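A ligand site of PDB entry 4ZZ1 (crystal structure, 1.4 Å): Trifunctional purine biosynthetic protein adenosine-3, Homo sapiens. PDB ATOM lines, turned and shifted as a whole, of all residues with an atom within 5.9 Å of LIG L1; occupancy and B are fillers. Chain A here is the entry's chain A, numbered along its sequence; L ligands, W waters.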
ATOM      1  N   LYS A  38       6.168 -18.920 -25.628  1.00  0.00           N
ATOM      2  CA  LYS A  38       5.730 -18.724 -27.008  1.00  0.00           C
ATOM      3  C   LYS A  38       6.590 -19.536 -27.965  1.00  0.00           C
ATOM      4  O   LYS A  38       7.812 -19.547 -27.874  1.00  0.00           O
ATOM      5  CB  LYS A  38       5.767 -17.246 -27.374  1.00  0.00           C
ATOM      6  CG  LYS A  38       4.687 -16.434 -26.678  1.00  0.00           C
ATOM      7  CD  LYS A  38       4.741 -14.969 -27.085  1.00  0.00           C
ATOM      8  CE  LYS A  38       3.620 -14.189 -26.428  1.00  0.00           C
ATOM      9  NZ  LYS A  38       3.712 -12.743 -26.737  1.00  0.00           N
ATOM     10  N   ARG A  65      -3.196 -18.886 -14.167  1.00  0.00           N
ATOM     11  CA  ARG A  65      -1.776 -18.671 -13.967  1.00  0.00           C
ATOM     12  C   ARG A  65      -1.140 -19.756 -13.116  1.00  0.00           C
ATOM     13  O   ARG A  65      -0.032 -20.203 -13.387  1.00  0.00           O
ATOM     14  CB  ARG A  65      -1.509 -17.298 -13.348  1.00  0.00           C
ATOM     15  CG  ARG A  65      -1.918 -16.149 -14.249  1.00  0.00           C
ATOM     16  CD  ARG A  65      -1.474 -14.789 -13.721  1.00  0.00           C
ATOM     17  NE  ARG A  65      -2.126 -13.730 -14.482  1.00  0.00           N
ATOM     18  CZ  ARG A  65      -1.634 -13.203 -15.594  1.00  0.00           C
ATOM     19  NH1 ARG A  65      -0.455 -13.587 -16.064  1.00  0.00           N
ATOM     20  NH2 ARG A  65      -2.328 -12.262 -16.225  1.00  0.00           N
ATOM     21  N   LEU A  86      14.188 -13.892 -15.617  1.00  0.00           N
ATOM     22  CA  LEU A  86      13.124 -13.514 -16.536  1.00  0.00           C
ATOM     23  C   LEU A  86      13.705 -12.489 -17.512  1.00  0.00           C
ATOM     24  O   LEU A  86      14.076 -11.394 -17.118  1.00  0.00           O
ATOM     25  CB  LEU A  86      11.926 -12.933 -15.774  1.00  0.00           C
ATOM     26  CG  LEU A  86      11.384 -13.770 -14.611  1.00  0.00           C
ATOM     27  CD1 LEU A  86      10.115 -13.121 -14.027  1.00  0.00           C
ATOM     28  CD2 LEU A  86      11.119 -15.213 -15.025  1.00  0.00           C
ATOM     29  N   PHE A  89      10.563 -12.175 -20.622  1.00  0.00           N
ATOM     30  CA  PHE A  89       9.394 -12.987 -20.299  1.00  0.00           C
ATOM     31  C   PHE A  89       8.241 -12.071 -19.894  1.00  0.00           C
ATOM     32  O   PHE A  89       8.412 -11.234 -18.997  1.00  0.00           O
ATOM     33  CB  PHE A  89       9.762 -13.948 -19.178  1.00  0.00           C
ATOM     34  CG  PHE A  89       8.663 -14.898 -18.794  1.00  0.00           C
ATOM     35  CD1 PHE A  89       8.340 -15.987 -19.588  1.00  0.00           C
ATOM     36  CD2 PHE A  89       7.967 -14.718 -17.599  1.00  0.00           C
ATOM     37  CE1 PHE A  89       7.345 -16.878 -19.209  1.00  0.00           C
ATOM     38  CE2 PHE A  89       6.969 -15.585 -17.216  1.00  0.00           C
ATOM     39  CZ  PHE A  89       6.656 -16.671 -18.024  1.00  0.00           C
ATOM     40  N   MET A  90       7.082 -12.210 -20.524  1.00  0.00           N
ATOM     41  CA  MET A  90       6.057 -11.173 -20.368  1.00  0.00           C
ATOM     42  C   MET A  90       4.836 -11.595 -19.547  1.00  0.00           C
ATOM     43  O   MET A  90       3.837 -10.856 -19.523  1.00  0.00           O
ATOM     44  CB  MET A  90       5.625 -10.666 -21.745  1.00  0.00           C
ATOM     45  CG  MET A  90       6.691  -9.844 -22.468  1.00  0.00           C
ATOM     46  SD  MET A  90       7.323  -8.418 -21.526  1.00  0.00           S
ATOM     47  CE  MET A  90       5.811  -7.508 -21.243  1.00  0.00           C
ATOM     48  N   ARG A  91       4.914 -12.725 -18.849  1.00  0.00           N
ATOM     49  CA  ARG A  91       3.782 -13.161 -18.023  1.00  0.00           C
ATOM     50  C   ARG A  91       3.945 -12.751 -16.568  1.00  0.00           C
ATOM     51  O   ARG A  91       5.027 -12.903 -15.975  1.00  0.00           O
ATOM     52  CB  ARG A  91       3.583 -14.673 -18.109  1.00  0.00           C
ATOM     53  CG  ARG A  91       3.344 -15.210 -19.513  1.00  0.00           C
ATOM     54  CD  ARG A  91       2.132 -14.575 -20.177  1.00  0.00           C
ATOM     55  NE  ARG A  91       0.881 -14.915 -19.492  1.00  0.00           N
ATOM     56  CZ  ARG A  91      -0.299 -14.410 -19.827  1.00  0.00           C
ATOM     57  NH1 ARG A  91      -0.405 -13.558 -20.834  1.00  0.00           N
ATOM     58  NH2 ARG A  91      -1.375 -14.775 -19.152  1.00  0.00           N
ATOM     59  N   ILE A  92       2.881 -12.218 -16.000  1.00  0.00           N
ATOM     60  CA  ILE A  92       2.763 -12.024 -14.567  1.00  0.00           C
ATOM     61  C   ILE A  92       2.678 -13.393 -13.890  1.00  0.00           C
ATOM     62  O   ILE A  92       1.839 -14.213 -14.274  1.00  0.00           O
ATOM     63  CB  ILE A  92       1.521 -11.176 -14.205  1.00  0.00           C
ATOM     64  CG1 ILE A  92       1.683  -9.771 -14.791  1.00  0.00           C
ATOM     65  CG2 ILE A  92       1.338 -11.123 -12.696  1.00  0.00           C
ATOM     66  CD1 ILE A  92       0.426  -8.918 -14.682  1.00  0.00           C
ATOM     67  N   LEU A  93       3.512 -13.625 -12.888  1.00  0.00           N
ATOM     68  CA  LEU A  93       3.572 -14.906 -12.190  1.00  0.00           C
ATOM     69  C   LEU A  93       2.697 -14.913 -10.952  1.00  0.00           C
ATOM     70  O   LEU A  93       2.507 -13.869 -10.317  1.00  0.00           O
ATOM     71  CB  LEU A  93       5.012 -15.236 -11.813  1.00  0.00           C
ATOM     72  CG  LEU A  93       5.945 -15.427 -13.011  1.00  0.00           C
ATOM     73  CD1 LEU A  93       7.389 -15.334 -12.547  1.00  0.00           C
ATOM     74  CD2 LEU A  93       5.661 -16.755 -13.694  1.00  0.00           C
ATOM     75  N   SER A  94       2.147 -16.082 -10.612  1.00  0.00           N
ATOM     76  CA  SER A  94       1.289 -16.226  -9.453  1.00  0.00           C
ATOM     77  C   SER A  94       2.049 -16.082  -8.139  1.00  0.00           C
ATOM     78  O   SER A  94       3.254 -16.329  -8.064  1.00  0.00           O
ATOM     79  CB  SER A  94       0.582 -17.590  -9.469  1.00  0.00           C
ATOM     80  OG  SER A  94       1.524 -18.634  -9.249  1.00  0.00           O
ATOM     81  N   GLY A  95       1.308 -15.715  -7.096  1.00  0.00           N
ATOM     82  CA  GLY A  95       1.873 -15.533  -5.768  1.00  0.00           C
ATOM     83  C   GLY A  95       2.674 -16.709  -5.225  1.00  0.00           C
ATOM     84  O   GLY A  95       3.811 -16.527  -4.796  1.00  0.00           O
ATOM     85  N   VAL A  98       6.026 -17.206  -7.067  1.00  0.00           N
ATOM     86  CA  VAL A  98       6.943 -16.139  -6.660  1.00  0.00           C
ATOM     87  C   VAL A  98       7.482 -16.388  -5.253  1.00  0.00           C
ATOM     88  O   VAL A  98       8.680 -16.245  -5.009  1.00  0.00           O
ATOM     89  CB  VAL A  98       6.241 -14.758  -6.743  1.00  0.00           C
ATOM     90  CG1 VAL A  98       7.087 -13.687  -6.082  1.00  0.00           C
ATOM     91  CG2 VAL A  98       5.935 -14.415  -8.197  1.00  0.00           C
ATOM     92  N   ASN A 107      14.432 -10.336 -12.546  1.00  0.00           N
ATOM     93  CA  ASN A 107      13.780  -9.790 -13.724  1.00  0.00           C
ATOM     94  C   ASN A 107      14.532  -8.586 -14.246  1.00  0.00           C
ATOM     95  O   ASN A 107      15.084  -7.818 -13.445  1.00  0.00           O
ATOM     96  CB  ASN A 107      12.333  -9.415 -13.399  1.00  0.00           C
ATOM     97  CG  ASN A 107      11.587  -8.867 -14.588  1.00  0.00           C
ATOM     98  OD1 ASN A 107      11.468  -9.524 -15.618  1.00  0.00           O
ATOM     99  ND2 ASN A 107      11.055  -7.644 -14.439  1.00  0.00           N
ATOM    100  N   HIS A 109      13.902  -5.051 -16.364  1.00  0.00           N
ATOM    101  CA  HIS A 109      12.806  -4.150 -16.699  1.00  0.00           C
ATOM    102  C   HIS A 109      13.408  -2.915 -17.355  1.00  0.00           C
ATOM    103  O   HIS A 109      14.355  -2.353 -16.812  1.00  0.00           O
ATOM    104  CB  HIS A 109      12.020  -3.788 -15.442  1.00  0.00           C
ATOM    105  CG  HIS A 109      10.859  -2.910 -15.740  1.00  0.00           C
ATOM    106  ND1 HIS A 109       9.658  -3.407 -16.203  1.00  0.00           N
ATOM    107  CD2 HIS A 109      10.724  -1.564 -15.685  1.00  0.00           C
ATOM    108  CE1 HIS A 109       8.828  -2.396 -16.414  1.00  0.00           C
ATOM    109  NE2 HIS A 109       9.452  -1.267 -16.100  1.00  0.00           N
ATOM    110  N   GLY A 118       5.311  -1.854 -15.645  1.00  0.00           N
ATOM    111  CA  GLY A 118       4.361  -2.421 -16.574  1.00  0.00           C
ATOM    112  C   GLY A 118       4.966  -2.834 -17.902  1.00  0.00           C
ATOM    113  O   GLY A 118       6.182  -2.955 -18.039  1.00  0.00           O
ATOM    114  N   SER A 119       4.103  -3.056 -18.901  1.00  0.00           N
ATOM    115  CA  SER A 119       4.527  -3.729 -20.119  1.00  0.00           C
ATOM    116  C   SER A 119       5.016  -2.814 -21.225  1.00  0.00           C
ATOM    117  O   SER A 119       5.579  -3.291 -22.216  1.00  0.00           O
ATOM    118  CB  SER A 119       3.364  -4.561 -20.680  1.00  0.00           C
ATOM    119  OG  SER A 119       2.303  -3.702 -21.042  1.00  0.00           O
ATOM    120  N   HIS A 138      15.876  -6.600 -10.797  1.00  0.00           N
ATOM    121  CA  HIS A 138      15.344  -6.696  -9.452  1.00  0.00           C
ATOM    122  C   HIS A 138      14.956  -8.127  -9.115  1.00  0.00           C
ATOM    123  O   HIS A 138      14.688  -8.936 -10.006  1.00  0.00           O
ATOM    124  CB  HIS A 138      14.130  -5.771  -9.265  1.00  0.00           C
ATOM    125  CG  HIS A 138      12.969  -6.106 -10.152  1.00  0.00           C
ATOM    126  ND1 HIS A 138      11.915  -6.892  -9.734  1.00  0.00           N
ATOM    127  CD2 HIS A 138      12.697  -5.771 -11.439  1.00  0.00           C
ATOM    128  CE1 HIS A 138      11.041  -7.012 -10.727  1.00  0.00           C
ATOM    129  NE2 HIS A 138      11.491  -6.347 -11.761  1.00  0.00           N
ATOM    130  N   PHE A 139      14.957  -8.453  -7.827  1.00  0.00           N
ATOM    131  CA  PHE A 139      14.341  -9.678  -7.359  1.00  0.00           C
ATOM    132  C   PHE A 139      12.844  -9.601  -7.622  1.00  0.00           C
ATOM    133  O   PHE A 139      12.222  -8.542  -7.452  1.00  0.00           O
ATOM    134  CB  PHE A 139      14.591  -9.898  -5.869  1.00  0.00           C
ATOM    135  CG  PHE A 139      15.988 -10.361  -5.545  1.00  0.00           C
ATOM    136  CD1 PHE A 139      16.389 -11.650  -5.869  1.00  0.00           C
ATOM    137  CD2 PHE A 139      16.888  -9.525  -4.889  1.00  0.00           C
ATOM    138  CE1 PHE A 139      17.683 -12.094  -5.567  1.00  0.00           C
ATOM    139  CE2 PHE A 139      18.169  -9.967  -4.581  1.00  0.00           C
ATOM    140  CZ  PHE A 139      18.567 -11.251  -4.913  1.00  0.00           C
ATOM    141  N   VAL A 140      12.254 -10.716  -8.015  1.00  0.00           N
ATOM    142  CA  VAL A 140      10.825 -10.759  -8.292  1.00  0.00           C
ATOM    143  C   VAL A 140      10.029 -10.961  -7.007  1.00  0.00           C
ATOM    144  O   VAL A 140      10.213 -11.953  -6.304  1.00  0.00           O
ATOM    145  CB  VAL A 140      10.493 -11.867  -9.304  1.00  0.00           C
ATOM    146  CG1 VAL A 140       8.977 -12.030  -9.459  1.00  0.00           C
ATOM    147  CG2 VAL A 140      11.140 -11.530 -10.645  1.00  0.00           C
ATOM    148  N   ALA A 141       9.152 -10.012  -6.716  1.00  0.00           N
ATOM    149  CA  ALA A 141       8.198 -10.112  -5.604  1.00  0.00           C
ATOM    150  C   ALA A 141       6.795 -10.245  -6.195  1.00  0.00           C
ATOM    151  O   ALA A 141       6.624 -10.079  -7.402  1.00  0.00           O
ATOM    152  CB  ALA A 141       8.300  -8.893  -4.704  1.00  0.00           C
ATOM    153  N   GLU A 142       5.793 -10.506  -5.361  1.00  0.00           N
ATOM    154  CA  GLU A 142       4.446 -10.712  -5.896  1.00  0.00           C
ATOM    155  C   GLU A 142       3.948  -9.475  -6.621  1.00  0.00           C
ATOM    156  O   GLU A 142       3.420  -9.565  -7.732  1.00  0.00           O
ATOM    157  CB  GLU A 142       3.474 -11.104  -4.783  1.00  0.00           C
ATOM    158  CG  GLU A 142       2.069 -11.348  -5.293  1.00  0.00           C
ATOM    159  CD  GLU A 142       1.217 -12.162  -4.340  1.00  0.00           C
ATOM    160  OE1 GLU A 142       1.757 -12.624  -3.301  1.00  0.00           O
ATOM    161  OE2 GLU A 142       0.014 -12.338  -4.615  1.00  0.00           O
ATOM    162  N   ASP A 143       4.094  -8.312  -5.997  1.00  0.00           N
ATOM    163  CA  ASP A 143       3.720  -7.064  -6.639  1.00  0.00           C
ATOM    164  C   ASP A 143       4.665  -6.831  -7.815  1.00  0.00           C
ATOM    165  O   ASP A 143       5.886  -6.795  -7.646  1.00  0.00           O
ATOM    166  CB  ASP A 143       3.757  -5.885  -5.664  1.00  0.00           C
ATOM    167  CG  ASP A 143       2.603  -5.910  -4.686  1.00  0.00           C
ATOM    168  OD1 ASP A 143       1.546  -6.486  -5.031  1.00  0.00           O
ATOM    169  OD2 ASP A 143       2.743  -5.345  -3.585  1.00  0.00           O
ATOM    170  N   VAL A 144       4.094  -6.669  -9.002  1.00  0.00           N
ATOM    171  CA  VAL A 144       4.865  -6.622 -10.236  1.00  0.00           C
ATOM    172  C   VAL A 144       5.790  -5.403 -10.310  1.00  0.00           C
ATOM    173  O   VAL A 144       5.381  -4.284 -10.026  1.00  0.00           O
ATOM    174  CB  VAL A 144       3.923  -6.641 -11.462  1.00  0.00           C
ATOM    175  CG1 VAL A 144       4.711  -6.505 -12.759  1.00  0.00           C
ATOM    176  CG2 VAL A 144       3.094  -7.932 -11.459  1.00  0.00           C
ATOM    177  N   ASP A 145       7.045  -5.648 -10.663  1.00  0.00           N
ATOM    178  CA  ASP A 145       8.055  -4.607 -10.856  1.00  0.00           C
ATOM    179  C   ASP A 145       8.331  -3.823  -9.575  1.00  0.00           C
ATOM    180  O   ASP A 145       8.765  -2.672  -9.631  1.00  0.00           O
ATOM    181  CB  ASP A 145       7.638  -3.642 -11.980  1.00  0.00           C
ATOM    182  CG  ASP A 145       7.571  -4.335 -13.338  1.00  0.00           C
ATOM    183  OD1 ASP A 145       8.209  -5.401 -13.507  1.00  0.00           O
ATOM    184  OD2 ASP A 145       6.907  -3.790 -14.251  1.00  0.00           O
ATOM    185  N   ALA A 146       8.104  -4.445  -8.416  1.00  0.00           N
ATOM    186  CA  ALA A 146       8.260  -3.774  -7.144  1.00  0.00           C
ATOM    187  C   ALA A 146       9.250  -4.463  -6.202  1.00  0.00           C
ATOM    188  O   ALA A 146       9.446  -3.994  -5.084  1.00  0.00           O
ATOM    189  CB  ALA A 146       6.904  -3.628  -6.452  1.00  0.00           C
ATOM    190  N   GLY A 147       9.847  -5.560  -6.647  1.00  0.00           N
ATOM    191  CA  GLY A 147      10.794  -6.285  -5.809  1.00  0.00           C
ATOM    192  C   GLY A 147      12.117  -5.561  -5.640  1.00  0.00           C
ATOM    193  O   GLY A 147      12.360  -4.521  -6.260  1.00  0.00           O
HETATM  194  N1  LIG L   1       5.369 -11.472 -11.861  1.00  0.00           N
HETATM  195  C1  LIG L   1       5.338 -11.021 -10.614  1.00  0.00           C
HETATM  196  N2  LIG L   1       6.163 -10.052 -10.182  1.00  0.00           N
HETATM  197  C2  LIG L   1       7.088  -9.493 -10.986  1.00  0.00           C
HETATM  198  N3  LIG L   1       6.487 -11.255 -14.022  1.00  0.00           N
HETATM  199  C3  LIG L   1       7.468 -10.508 -14.509  1.00  0.00           C
HETATM  200  C4  LIG L   1       7.949  -9.660 -13.493  1.00  0.00           C
HETATM  201  C5  LIG L   1       7.165  -9.953 -12.344  1.00  0.00           C
HETATM  202  C6  LIG L   1       6.267 -10.975 -12.743  1.00  0.00           C
HETATM  203  O1  LIG L   1       7.845  -8.609 -10.579  1.00  0.00           O
HETATM  204  N4  LIG L   1       4.403 -11.556  -9.728  1.00  0.00           N
HETATM  205  C7  LIG L   1       4.019  -8.401 -17.233  1.00  0.00           C
HETATM  206  C8  LIG L   1       2.966  -7.617 -17.619  1.00  0.00           C
HETATM  207  S1  LIG L   1       3.406  -6.021 -17.242  1.00  0.00           S
HETATM  208  C9  LIG L   1       4.948  -6.368 -16.593  1.00  0.00           C
HETATM  209  C10 LIG L   1       5.135  -7.727 -16.664  1.00  0.00           C
HETATM  210  C11 LIG L   1       1.724  -8.012 -18.214  1.00  0.00           C
HETATM  211  O2  LIG L   1       0.783  -7.200 -18.292  1.00  0.00           O
HETATM  212  N5  LIG L   1       1.605  -9.352 -18.710  1.00  0.00           N
HETATM  213  C12 LIG L   1       0.358  -9.758 -19.296  1.00  0.00           C
HETATM  214  C13 LIG L   1       0.602 -10.171 -20.704  1.00  0.00           C
HETATM  215  C14 LIG L   1       0.786  -8.949 -21.598  1.00  0.00           C
HETATM  216  C15 LIG L   1       1.462  -9.308 -22.946  1.00  0.00           C
HETATM  217  O3  LIG L   1       2.293  -8.484 -23.487  1.00  0.00           O
HETATM  218  O4  LIG L   1       1.189 -10.447 -23.529  1.00  0.00           O
HETATM  219  C16 LIG L   1      -0.166 -10.934 -18.474  1.00  0.00           C
HETATM  220  O5  LIG L   1      -1.453 -11.138 -18.398  1.00  0.00           O
HETATM  221  O6  LIG L   1       0.658 -11.701 -17.849  1.00  0.00           O
HETATM  222  C17 LIG L   1       7.911 -10.571 -15.991  1.00  0.00           C
HETATM  223  C18 LIG L   1       6.768  -9.803 -16.787  1.00  0.00           C
HETATM  224  C19 LIG L   1       6.385  -8.441 -16.151  1.00  0.00           C
HETATM  225  C1  LG2 L   2      13.767  -6.085 -22.935  1.00  0.00           C
HETATM  226  O1  LG2 L   2      13.847  -4.678 -23.239  1.00  0.00           O
HETATM  227  C2  LG2 L   2      13.255  -6.291 -21.530  1.00  0.00           C
HETATM  228  O2  LG2 L   2      13.778  -5.396 -20.527  1.00  0.00           O
HETATM  229  C3  LG2 L   2      11.766  -6.084 -21.740  1.00  0.00           C
HETATM  230  O3  LG2 L   2      11.515  -6.804 -22.930  1.00  0.00           O
HETATM  231  C4  LG2 L   2      12.663  -6.719 -23.781  1.00  0.00           C
HETATM  232  C5  LG2 L   2      13.026  -8.150 -24.178  1.00  0.00           C
HETATM  233  O4  LG2 L   2      14.061  -8.119 -25.155  1.00  0.00           O
HETATM  234  N1  LG2 L   2      10.991  -6.640 -20.658  1.00  0.00           N
HETATM  235  C6  LG2 L   2       9.862  -6.086 -20.225  1.00  0.00           C
HETATM  236  O5  LG2 L   2       9.309  -5.120 -20.761  1.00  0.00           O
HETATM  237  C7  LG2 L   2       9.330  -6.752 -18.973  1.00  0.00           C
HETATM  238  N2  LG2 L   2       8.049  -6.255 -18.552  1.00  0.00           N
HETATM  239  P1  LG2 L   2      14.874  -9.485 -25.492  1.00  0.00           P
HETATM  240  O6  LG2 L   2      15.711  -9.784 -24.272  1.00  0.00           O
HETATM  241  O7  LG2 L   2      15.689  -9.088 -26.713  1.00  0.00           O
HETATM  242  O8  LG2 L   2      13.842 -10.564 -25.773  1.00  0.00           O
HETATM  243  O   HOH W   1      -0.298  -5.251 -19.859  1.00  0.00           O
HETATM  244  O   HOH W   2       0.253  -5.207 -16.463  1.00  0.00           O
HETATM  245  O   HOH W   3       4.210  -9.098 -25.115  1.00  0.00           O
HETATM  246  O   HOH W   4       8.482  -7.624  -8.175  1.00  0.00           O
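The guanidinium group (NH2) of Arg 65 is in salt-bridge range of an oxygen (O5) of LIG L1 (2.6 Å). The backbone carbonyl oxygen of Met 90 lies within hydrogen-bond range of a nitrogen (N5) of LIG L1, 2.8 Å away. The backbone carbonyl oxygen of Ala 141 sits at hydrogen-bond distance from a nitrogen (N2) of LIG L1 (2.8 Å). The backbone NH (N) of Ile 92 is in hydrogen-bond range of an oxygen (O6) of LIG L1 (2.9 Å). O of Arg 91 sits at hydrogen-bond distance from N3 of LIG L1, 2.9 Å away. The guanidinium group of Arg 91 lies within salt-bridge range of an oxygen (O5) of LIG L1, at 3.6 Å. The backbone carbonyl oxygen (O) of Glu 142 sits at hydrogen-bond distance from a nitrogen (N4) of LIG L1 (3.0 Å). A nitrogen (N1) of LIG L1 lies within hydrogen-bond range of the backbone NH (N) of Leu 93 (3.0 Å). A nitrogen (N4) of LIG L1 sits at hydrogen-bond distance from the backbone carbonyl oxygen (O) of Leu 93. An oxygen (O1) of LIG L1 is in hydrogen-bond range of the backbone NH (N) of Asp 145 (3.1 Å). N of Ser 119 sits close to S1 of LIG L1 (3.5 Å). The side-chain sulfur (SD) of Met 90 lies close to a nitrogen (N2) of LG2 L2, at 3.7 Å.
Water W1 lies within hydrogen-bond range of an oxygen (O2) of LIG L1 and the side-chain hydroxyl (OG) of Ser 119.
NH1 of Arg 65 is in hydrogen-bond range of O of Ile 92 (3.0 Å). The backbone NH of Gly 118 is in hydrogen-bond range of the side-chain carboxylate of Asp 145. A ring nitrogen (ND1) of His 109 sits close to the side-chain carboxylate of Asp 145, 3.4 Å away. The backbone carbonyl oxygen (O) of His 138 is in hydrogen-bond range of the backbone NH (N) of Asn 107 (2.9 Å).
Leu 86 touches LIG L1 (CD1 to C3, 3.8 Å). Phe 89 touches LIG L1 (O to C18, 3.1 Å). CG2 of Val 98 touches N4 of LIG L1 (3.6 Å). Asn 107 touches LIG L1. C of Gly 118 touches S1 of LIG L1 (3.6 Å). CE1 of His 138 touches O1 of LIG L1, 3.6 Å away. Val 140 touches LIG L1. Asp 143 touches LIG L1 (O to O1, 3.97 Å). Val 144 touches LIG L1. Within 4 Å of LIG L1: Arg 65, Leu 86, Phe 89, Met 90, Arg 91, Ile 92, Leu 93, Val 98, Asn 107, Gly 118, Ser 119, His 138, Val 140, Ala 141, Glu 142, Asp 143, Val 144 and Asp 145. The nearest printed residue that does not touch LIG L1 is Lys 38 (4.7 Å).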
